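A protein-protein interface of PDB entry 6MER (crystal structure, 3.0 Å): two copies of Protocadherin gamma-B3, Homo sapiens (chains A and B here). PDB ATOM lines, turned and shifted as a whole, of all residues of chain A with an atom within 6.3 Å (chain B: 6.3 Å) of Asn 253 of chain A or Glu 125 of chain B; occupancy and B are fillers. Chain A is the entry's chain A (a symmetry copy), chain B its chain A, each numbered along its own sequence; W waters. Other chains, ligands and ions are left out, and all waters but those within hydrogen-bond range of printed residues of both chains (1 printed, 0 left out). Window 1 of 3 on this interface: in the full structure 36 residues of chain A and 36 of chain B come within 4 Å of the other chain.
The side-chain hydroxyl (OG) of Ser 104 of chain B lies within hydrogen-bond range of the backbone carbonyl oxygen (O) of Ile 254 of chain A (3.4 Å).
ND2 of Asn 253 of chain A sits at hydrogen-bond distance from OG of Ser 126 of chain B (2.9 Å).
The side-chain hydroxyl of Ser 104 of chain B is in hydrogen-bond range of the side-chain carboxylate of Glu 125 of chain B (2.7 Å).
Among the printed residues, pairs that only touch across the chains: Gly 255 of chain A with Gln 128 of chain B (3.3 Å), Ile 254 of chain A with Glu 125 of chain B (3.7 Å) and Asn 253 of chain A with Glu 125 of chain B (3.99 Å).
Of the printed residues of chain B, Asn 253 of chain A touches Glu 125 (3.99 Å) and Ser 126 (2.9 Å).
Printed residues of chain A within 4 Å of Glu 125 of chain B: Asn 253 and Ile 254.
Printed residues of chain A within 4 Å of Ser 126 of chain B: Asn 253.
Of the printed residues of chain B, Ile 254 of chain A touches Ser 104 (3.4 Å) and Glu 125 (3.7 Å).
Gln 105 of chain B touches none of the printed residues of chain A.
The nearest printed residue of chain B that does not touch Asn 253 of chain A is Leu 124 of chain B (4.4 Å).
The nearest printed residue of chain A that does not touch Glu 125 of chain B is Arg 259 of chain A (4.3 Å).
Of the 8 printed residues of chain A, 3 touch a printed residue of chain B.
Printed residues of chain B that touch a printed residue of chain A: Ser 104, Glu 125, Ser 126 and Gln 128.
Among the printed residues, no Asp or Glu carboxylate lies within 4 Å of a Lys or Arg side-chain nitrogen of the other chain.
No position is printed for both chains.
Of the 5 pairs that touch across the chains among the printed residues, none has its exchanged pair printed and touching as well.
Water W1 bridges the side-chain carboxylate of Glu 125 of chain B (2.7 Å) and the guanidinium group of Arg 259 of chain A (3.4 Å).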
ATOM      1  N   PHE A 251      -2.184  12.182  11.741  1.00  0.00           N
ATOM      2  CA  PHE A 251      -2.598  11.051  10.926  1.00  0.00           C
ATOM      3  C   PHE A 251      -2.547   9.760  11.732  1.00  0.00           C
ATOM      4  O   PHE A 251      -1.714   9.591  12.627  1.00  0.00           O
ATOM      5  CB  PHE A 251      -1.705  10.925   9.690  1.00  0.00           C
ATOM      6  CG  PHE A 251      -1.921  12.006   8.669  1.00  0.00           C
ATOM      7  CD1 PHE A 251      -3.149  12.635   8.554  1.00  0.00           C
ATOM      8  CD2 PHE A 251      -0.895  12.390   7.822  1.00  0.00           C
ATOM      9  CE1 PHE A 251      -3.350  13.626   7.610  1.00  0.00           C
ATOM     10  CE2 PHE A 251      -1.088  13.381   6.879  1.00  0.00           C
ATOM     11  CZ  PHE A 251      -2.317  13.999   6.772  1.00  0.00           C
ATOM     12  N   ILE A 252      -3.453   8.841  11.402  1.00  0.00           N
ATOM     13  CA  ILE A 252      -3.534   7.545  12.061  1.00  0.00           C
ATOM     14  C   ILE A 252      -3.635   6.456  11.004  1.00  0.00           C
ATOM     15  O   ILE A 252      -4.226   6.654   9.936  1.00  0.00           O
ATOM     16  CB  ILE A 252      -4.732   7.458  13.032  1.00  0.00           C
ATOM     17  CG1 ILE A 252      -6.026   7.834  12.308  1.00  0.00           C
ATOM     18  CG2 ILE A 252      -4.502   8.342  14.247  1.00  0.00           C
ATOM     19  CD1 ILE A 252      -7.275   7.480  13.070  1.00  0.00           C
ATOM     20  N   ASN A 253      -3.052   5.298  11.314  1.00  0.00           N
ATOM     21  CA  ASN A 253      -3.103   4.122  10.445  1.00  0.00           C
ATOM     22  C   ASN A 253      -2.604   4.459   9.042  1.00  0.00           C
ATOM     23  O   ASN A 253      -3.247   4.160   8.033  1.00  0.00           O
ATOM     24  CB  ASN A 253      -4.516   3.537  10.405  1.00  0.00           C
ATOM     25  CG  ASN A 253      -4.534   2.077   9.998  1.00  0.00           C
ATOM     26  OD1 ASN A 253      -3.666   1.612   9.258  1.00  0.00           O
ATOM     27  ND2 ASN A 253      -5.530   1.343  10.481  1.00  0.00           N
ATOM     28  N   ILE A 254      -1.438   5.098   8.986  1.00  0.00           N
ATOM     29  CA  ILE A 254      -0.860   5.554   7.732  1.00  0.00           C
ATOM     30  C   ILE A 254       0.488   4.871   7.535  1.00  0.00           C
ATOM     31  O   ILE A 254       1.119   4.394   8.483  1.00  0.00           O
ATOM     32  CB  ILE A 254      -0.713   7.091   7.689  1.00  0.00           C
ATOM     33  CG1 ILE A 254      -0.838   7.600   6.253  1.00  0.00           C
ATOM     34  CG2 ILE A 254       0.608   7.529   8.308  1.00  0.00           C
ATOM     35  CD1 ILE A 254      -2.172   7.280   5.613  1.00  0.00           C
ATOM     36  N   GLY A 255       0.923   4.818   6.276  1.00  0.00           N
ATOM     37  CA  GLY A 255       2.179   4.207   5.909  1.00  0.00           C
ATOM     38  C   GLY A 255       3.140   5.206   5.286  1.00  0.00           C
ATOM     39  O   GLY A 255       2.810   6.374   5.061  1.00  0.00           O
ATOM     40  N   ARG A 259       2.912   8.958   4.129  1.00  0.00           N
ATOM     41  CA  ARG A 259       3.609   9.842   5.057  1.00  0.00           C
ATOM     42  C   ARG A 259       4.617  10.725   4.331  1.00  0.00           C
ATOM     43  O   ARG A 259       4.821  11.885   4.708  1.00  0.00           O
ATOM     44  CB  ARG A 259       4.297   9.017   6.144  1.00  0.00           C
ATOM     45  CG  ARG A 259       4.923   9.837   7.258  1.00  0.00           C
ATOM     46  CD  ARG A 259       5.403   8.936   8.384  1.00  0.00           C
ATOM     47  NE  ARG A 259       4.327   8.085   8.885  1.00  0.00           N
ATOM     48  CZ  ARG A 259       4.470   7.195   9.861  1.00  0.00           C
ATOM     49  NH1 ARG A 259       5.647   7.037  10.450  1.00  0.00           N
ATOM     50  NH2 ARG A 259       3.434   6.464  10.250  1.00  0.00           N
ATOM     51  N   THR A 286      -6.883   7.635   0.959  1.00  0.00           N
ATOM     52  CA  THR A 286      -7.802   7.632   2.093  1.00  0.00           C
ATOM     53  C   THR A 286      -6.974   7.681   3.369  1.00  0.00           C
ATOM     54  O   THR A 286      -6.256   6.726   3.687  1.00  0.00           O
ATOM     55  CB  THR A 286      -8.708   6.400   2.072  1.00  0.00           C
ATOM     56  OG1 THR A 286      -9.568   6.458   0.926  1.00  0.00           O
ATOM     57  CG2 THR A 286      -9.555   6.340   3.334  1.00  0.00           C
ATOM     58  N   GLY A 288      -6.801   8.679   7.619  1.00  0.00           N
ATOM     59  CA  GLY A 288      -7.524   8.872   8.864  1.00  0.00           C
ATOM     60  C   GLY A 288      -6.898   9.992   9.677  1.00  0.00           C
ATOM     61  O   GLY A 288      -5.676  10.088   9.783  1.00  0.00           O
ATOM     62  N   PHE B 103       4.363  -3.410  11.361  1.00  0.00           N
ATOM     63  CA  PHE B 103       3.797  -2.254  12.038  1.00  0.00           C
ATOM     64  C   PHE B 103       4.672  -1.030  11.792  1.00  0.00           C
ATOM     65  O   PHE B 103       5.859  -1.138  11.474  1.00  0.00           O
ATOM     66  CB  PHE B 103       3.658  -2.513  13.540  1.00  0.00           C
ATOM     67  CG  PHE B 103       2.575  -3.494  13.890  1.00  0.00           C
ATOM     68  CD1 PHE B 103       2.862  -4.841  14.044  1.00  0.00           C
ATOM     69  CD2 PHE B 103       1.268  -3.069  14.069  1.00  0.00           C
ATOM     70  CE1 PHE B 103       1.866  -5.744  14.369  1.00  0.00           C
ATOM     71  CE2 PHE B 103       0.268  -3.968  14.393  1.00  0.00           C
ATOM     72  CZ  PHE B 103       0.568  -5.307  14.544  1.00  0.00           C
ATOM     73  N   SER B 104       4.065   0.150  11.943  1.00  0.00           N
ATOM     74  CA  SER B 104       4.793   1.388  11.684  1.00  0.00           C
ATOM     75  C   SER B 104       5.938   1.587  12.667  1.00  0.00           C
ATOM     76  O   SER B 104       6.933   2.242  12.336  1.00  0.00           O
ATOM     77  CB  SER B 104       3.837   2.579  11.735  1.00  0.00           C
ATOM     78  OG  SER B 104       2.810   2.452  10.767  1.00  0.00           O
ATOM     79  N   GLN B 105       5.820   1.035  13.872  1.00  0.00           N
ATOM     80  CA  GLN B 105       6.853   1.179  14.888  1.00  0.00           C
ATOM     81  C   GLN B 105       6.811  -0.027  15.813  1.00  0.00           C
ATOM     82  O   GLN B 105       5.737  -0.557  16.107  1.00  0.00           O
ATOM     83  CB  GLN B 105       6.671   2.478  15.681  1.00  0.00           C
ATOM     84  CG  GLN B 105       5.240   2.742  16.116  1.00  0.00           C
ATOM     85  CD  GLN B 105       5.024   4.174  16.563  1.00  0.00           C
ATOM     86  OE1 GLN B 105       5.957   4.976  16.586  1.00  0.00           O
ATOM     87  NE2 GLN B 105       3.786   4.502  16.915  1.00  0.00           N
ATOM     88  N   THR B 108       4.751   1.228  20.494  1.00  0.00           N
ATOM     89  CA  THR B 108       3.780   2.310  20.411  1.00  0.00           C
ATOM     90  C   THR B 108       3.269   2.634  21.808  1.00  0.00           C
ATOM     91  O   THR B 108       3.054   1.732  22.623  1.00  0.00           O
ATOM     92  CB  THR B 108       2.607   1.931  19.496  1.00  0.00           C
ATOM     93  OG1 THR B 108       3.111   1.458  18.240  1.00  0.00           O
ATOM     94  CG2 THR B 108       1.705   3.132  19.248  1.00  0.00           C
ATOM     95  N   ALA B 123      -8.618   3.057  19.507  1.00  0.00           N
ATOM     96  CA  ALA B 123      -8.176   2.663  18.177  1.00  0.00           C
ATOM     97  C   ALA B 123      -6.703   2.269  18.184  1.00  0.00           C
ATOM     98  O   ALA B 123      -5.873   2.905  18.840  1.00  0.00           O
ATOM     99  CB  ALA B 123      -8.409   3.798  17.181  1.00  0.00           C
ATOM    100  N   LEU B 124      -6.386   1.211  17.445  1.00  0.00           N
ATOM    101  CA  LEU B 124      -5.023   0.737  17.268  1.00  0.00           C
ATOM    102  C   LEU B 124      -4.602   0.898  15.814  1.00  0.00           C
ATOM    103  O   LEU B 124      -5.434   1.015  14.910  1.00  0.00           O
ATOM    104  CB  LEU B 124      -4.889  -0.732  17.688  1.00  0.00           C
ATOM    105  CG  LEU B 124      -5.173  -1.068  19.152  1.00  0.00           C
ATOM    106  CD1 LEU B 124      -5.067  -2.567  19.379  1.00  0.00           C
ATOM    107  CD2 LEU B 124      -4.223  -0.316  20.069  1.00  0.00           C
ATOM    108  N   GLU B 125      -3.290   0.903  15.596  1.00  0.00           N
ATOM    109  CA  GLU B 125      -2.735   1.027  14.256  1.00  0.00           C
ATOM    110  C   GLU B 125      -2.646  -0.348  13.609  1.00  0.00           C
ATOM    111  O   GLU B 125      -2.101  -1.287  14.200  1.00  0.00           O
ATOM    112  CB  GLU B 125      -1.355   1.686  14.296  1.00  0.00           C
ATOM    113  CG  GLU B 125      -0.793   2.011  12.922  1.00  0.00           C
ATOM    114  CD  GLU B 125       0.521   2.761  12.992  1.00  0.00           C
ATOM    115  OE1 GLU B 125       1.279   2.552  13.964  1.00  0.00           O
ATOM    116  OE2 GLU B 125       0.793   3.567  12.077  1.00  0.00           O
ATOM    117  N   SER B 126      -3.185  -0.463  12.400  1.00  0.00           N
ATOM    118  CA  SER B 126      -3.182  -1.730  11.689  1.00  0.00           C
ATOM    119  C   SER B 126      -1.817  -1.996  11.065  1.00  0.00           C
ATOM    120  O   SER B 126      -1.011  -1.086  10.849  1.00  0.00           O
ATOM    121  CB  SER B 126      -4.261  -1.742  10.607  1.00  0.00           C
ATOM    122  OG  SER B 126      -5.533  -1.444  11.152  1.00  0.00           O
ATOM    123  N   ALA B 127      -1.564  -3.268  10.777  1.00  0.00           N
ATOM    124  CA  ALA B 127      -0.335  -3.679  10.116  1.00  0.00           C
ATOM    125  C   ALA B 127      -0.521  -3.649   8.607  1.00  0.00           C
ATOM    126  O   ALA B 127      -1.604  -3.949   8.095  1.00  0.00           O
ATOM    127  CB  ALA B 127       0.079  -5.081  10.568  1.00  0.00           C
ATOM    128  N   GLN B 128       0.539  -3.278   7.898  1.00  0.00           N
ATOM    129  CA  GLN B 128       0.526  -3.223   6.444  1.00  0.00           C
ATOM    130  C   GLN B 128       1.189  -4.468   5.871  1.00  0.00           C
ATOM    131  O   GLN B 128       2.187  -4.957   6.408  1.00  0.00           O
ATOM    132  CB  GLN B 128       1.238  -1.969   5.936  1.00  0.00           C
ATOM    133  CG  GLN B 128       0.506  -0.674   6.243  1.00  0.00           C
ATOM    134  CD  GLN B 128       1.234   0.544   5.710  1.00  0.00           C
ATOM    135  OE1 GLN B 128       2.323   0.885   6.174  1.00  0.00           O
ATOM    136  NE2 GLN B 128       0.636   1.208   4.726  1.00  0.00           N
ATOM    137  N   TYR B 140      -5.447 -10.410  14.055  1.00  0.00           N
ATOM    138  CA  TYR B 140      -4.800  -9.718  15.162  1.00  0.00           C
ATOM    139  C   TYR B 140      -5.073 -10.447  16.470  1.00  0.00           C
ATOM    140  O   TYR B 140      -6.226 -10.756  16.787  1.00  0.00           O
ATOM    141  CB  TYR B 140      -5.279  -8.268  15.248  1.00  0.00           C
ATOM    142  CG  TYR B 140      -4.888  -7.441  14.045  1.00  0.00           C
ATOM    143  CD1 TYR B 140      -3.663  -6.791  13.995  1.00  0.00           C
ATOM    144  CD2 TYR B 140      -5.740  -7.321  12.955  1.00  0.00           C
ATOM    145  CE1 TYR B 140      -3.299  -6.037  12.897  1.00  0.00           C
ATOM    146  CE2 TYR B 140      -5.384  -6.569  11.851  1.00  0.00           C
ATOM    147  CZ  TYR B 140      -4.162  -5.929  11.828  1.00  0.00           C
ATOM    148  OH  TYR B 140      -3.804  -5.180  10.732  1.00  0.00           O
ATOM    149  N   TYR B 161      -9.017  -4.612  11.076  1.00  0.00           N
ATOM    150  CA  TYR B 161      -8.261  -3.693  11.908  1.00  0.00           C
ATOM    151  C   TYR B 161      -8.551  -3.968  13.377  1.00  0.00           C
ATOM    152  O   TYR B 161      -9.697  -4.259  13.741  1.00  0.00           O
ATOM    153  CB  TYR B 161      -8.598  -2.231  11.571  1.00  0.00           C
ATOM    154  CG  TYR B 161     -10.035  -1.839  11.838  1.00  0.00           C
ATOM    155  CD1 TYR B 161     -10.395  -1.204  13.020  1.00  0.00           C
ATOM    156  CD2 TYR B 161     -11.031  -2.099  10.905  1.00  0.00           C
ATOM    157  CE1 TYR B 161     -11.706  -0.843  13.267  1.00  0.00           C
ATOM    158  CE2 TYR B 161     -12.344  -1.742  11.144  1.00  0.00           C
ATOM    159  CZ  TYR B 161     -12.676  -1.114  12.326  1.00  0.00           C
ATOM    160  OH  TYR B 161     -13.982  -0.755  12.568  1.00  0.00           O
ATOM    161  N   PRO B 162      -7.540  -3.895  14.237  1.00  0.00           N
ATOM    162  CA  PRO B 162      -7.752  -4.153  15.663  1.00  0.00           C
ATOM    163  C   PRO B 162      -8.162  -2.907  16.432  1.00  0.00           C
ATOM    164  O   PRO B 162      -7.836  -1.774  16.071  1.00  0.00           O
ATOM    165  CB  PRO B 162      -6.374  -4.646  16.122  1.00  0.00           C
ATOM    166  CG  PRO B 162      -5.426  -3.887  15.253  1.00  0.00           C
ATOM    167  CD  PRO B 162      -6.114  -3.711  13.917  1.00  0.00           C
ATOM    168  N   LEU B 182       0.945  -6.966  20.658  1.00  0.00           N
ATOM    169  CA  LEU B 182      -0.013  -7.176  19.581  1.00  0.00           C
ATOM    170  C   LEU B 182       0.680  -7.882  18.423  1.00  0.00           C
ATOM    171  O   LEU B 182       1.741  -7.441  17.969  1.00  0.00           O
ATOM    172  CB  LEU B 182      -0.614  -5.849  19.114  1.00  0.00           C
ATOM    173  CG  LEU B 182      -1.668  -5.938  18.009  1.00  0.00           C
ATOM    174  CD1 LEU B 182      -2.831  -6.812  18.450  1.00  0.00           C
ATOM    175  CD2 LEU B 182      -2.152  -4.550  17.617  1.00  0.00           C
HETATM  176  O   HOH W   1       0.561   6.259  11.967  1.00  0.00           O
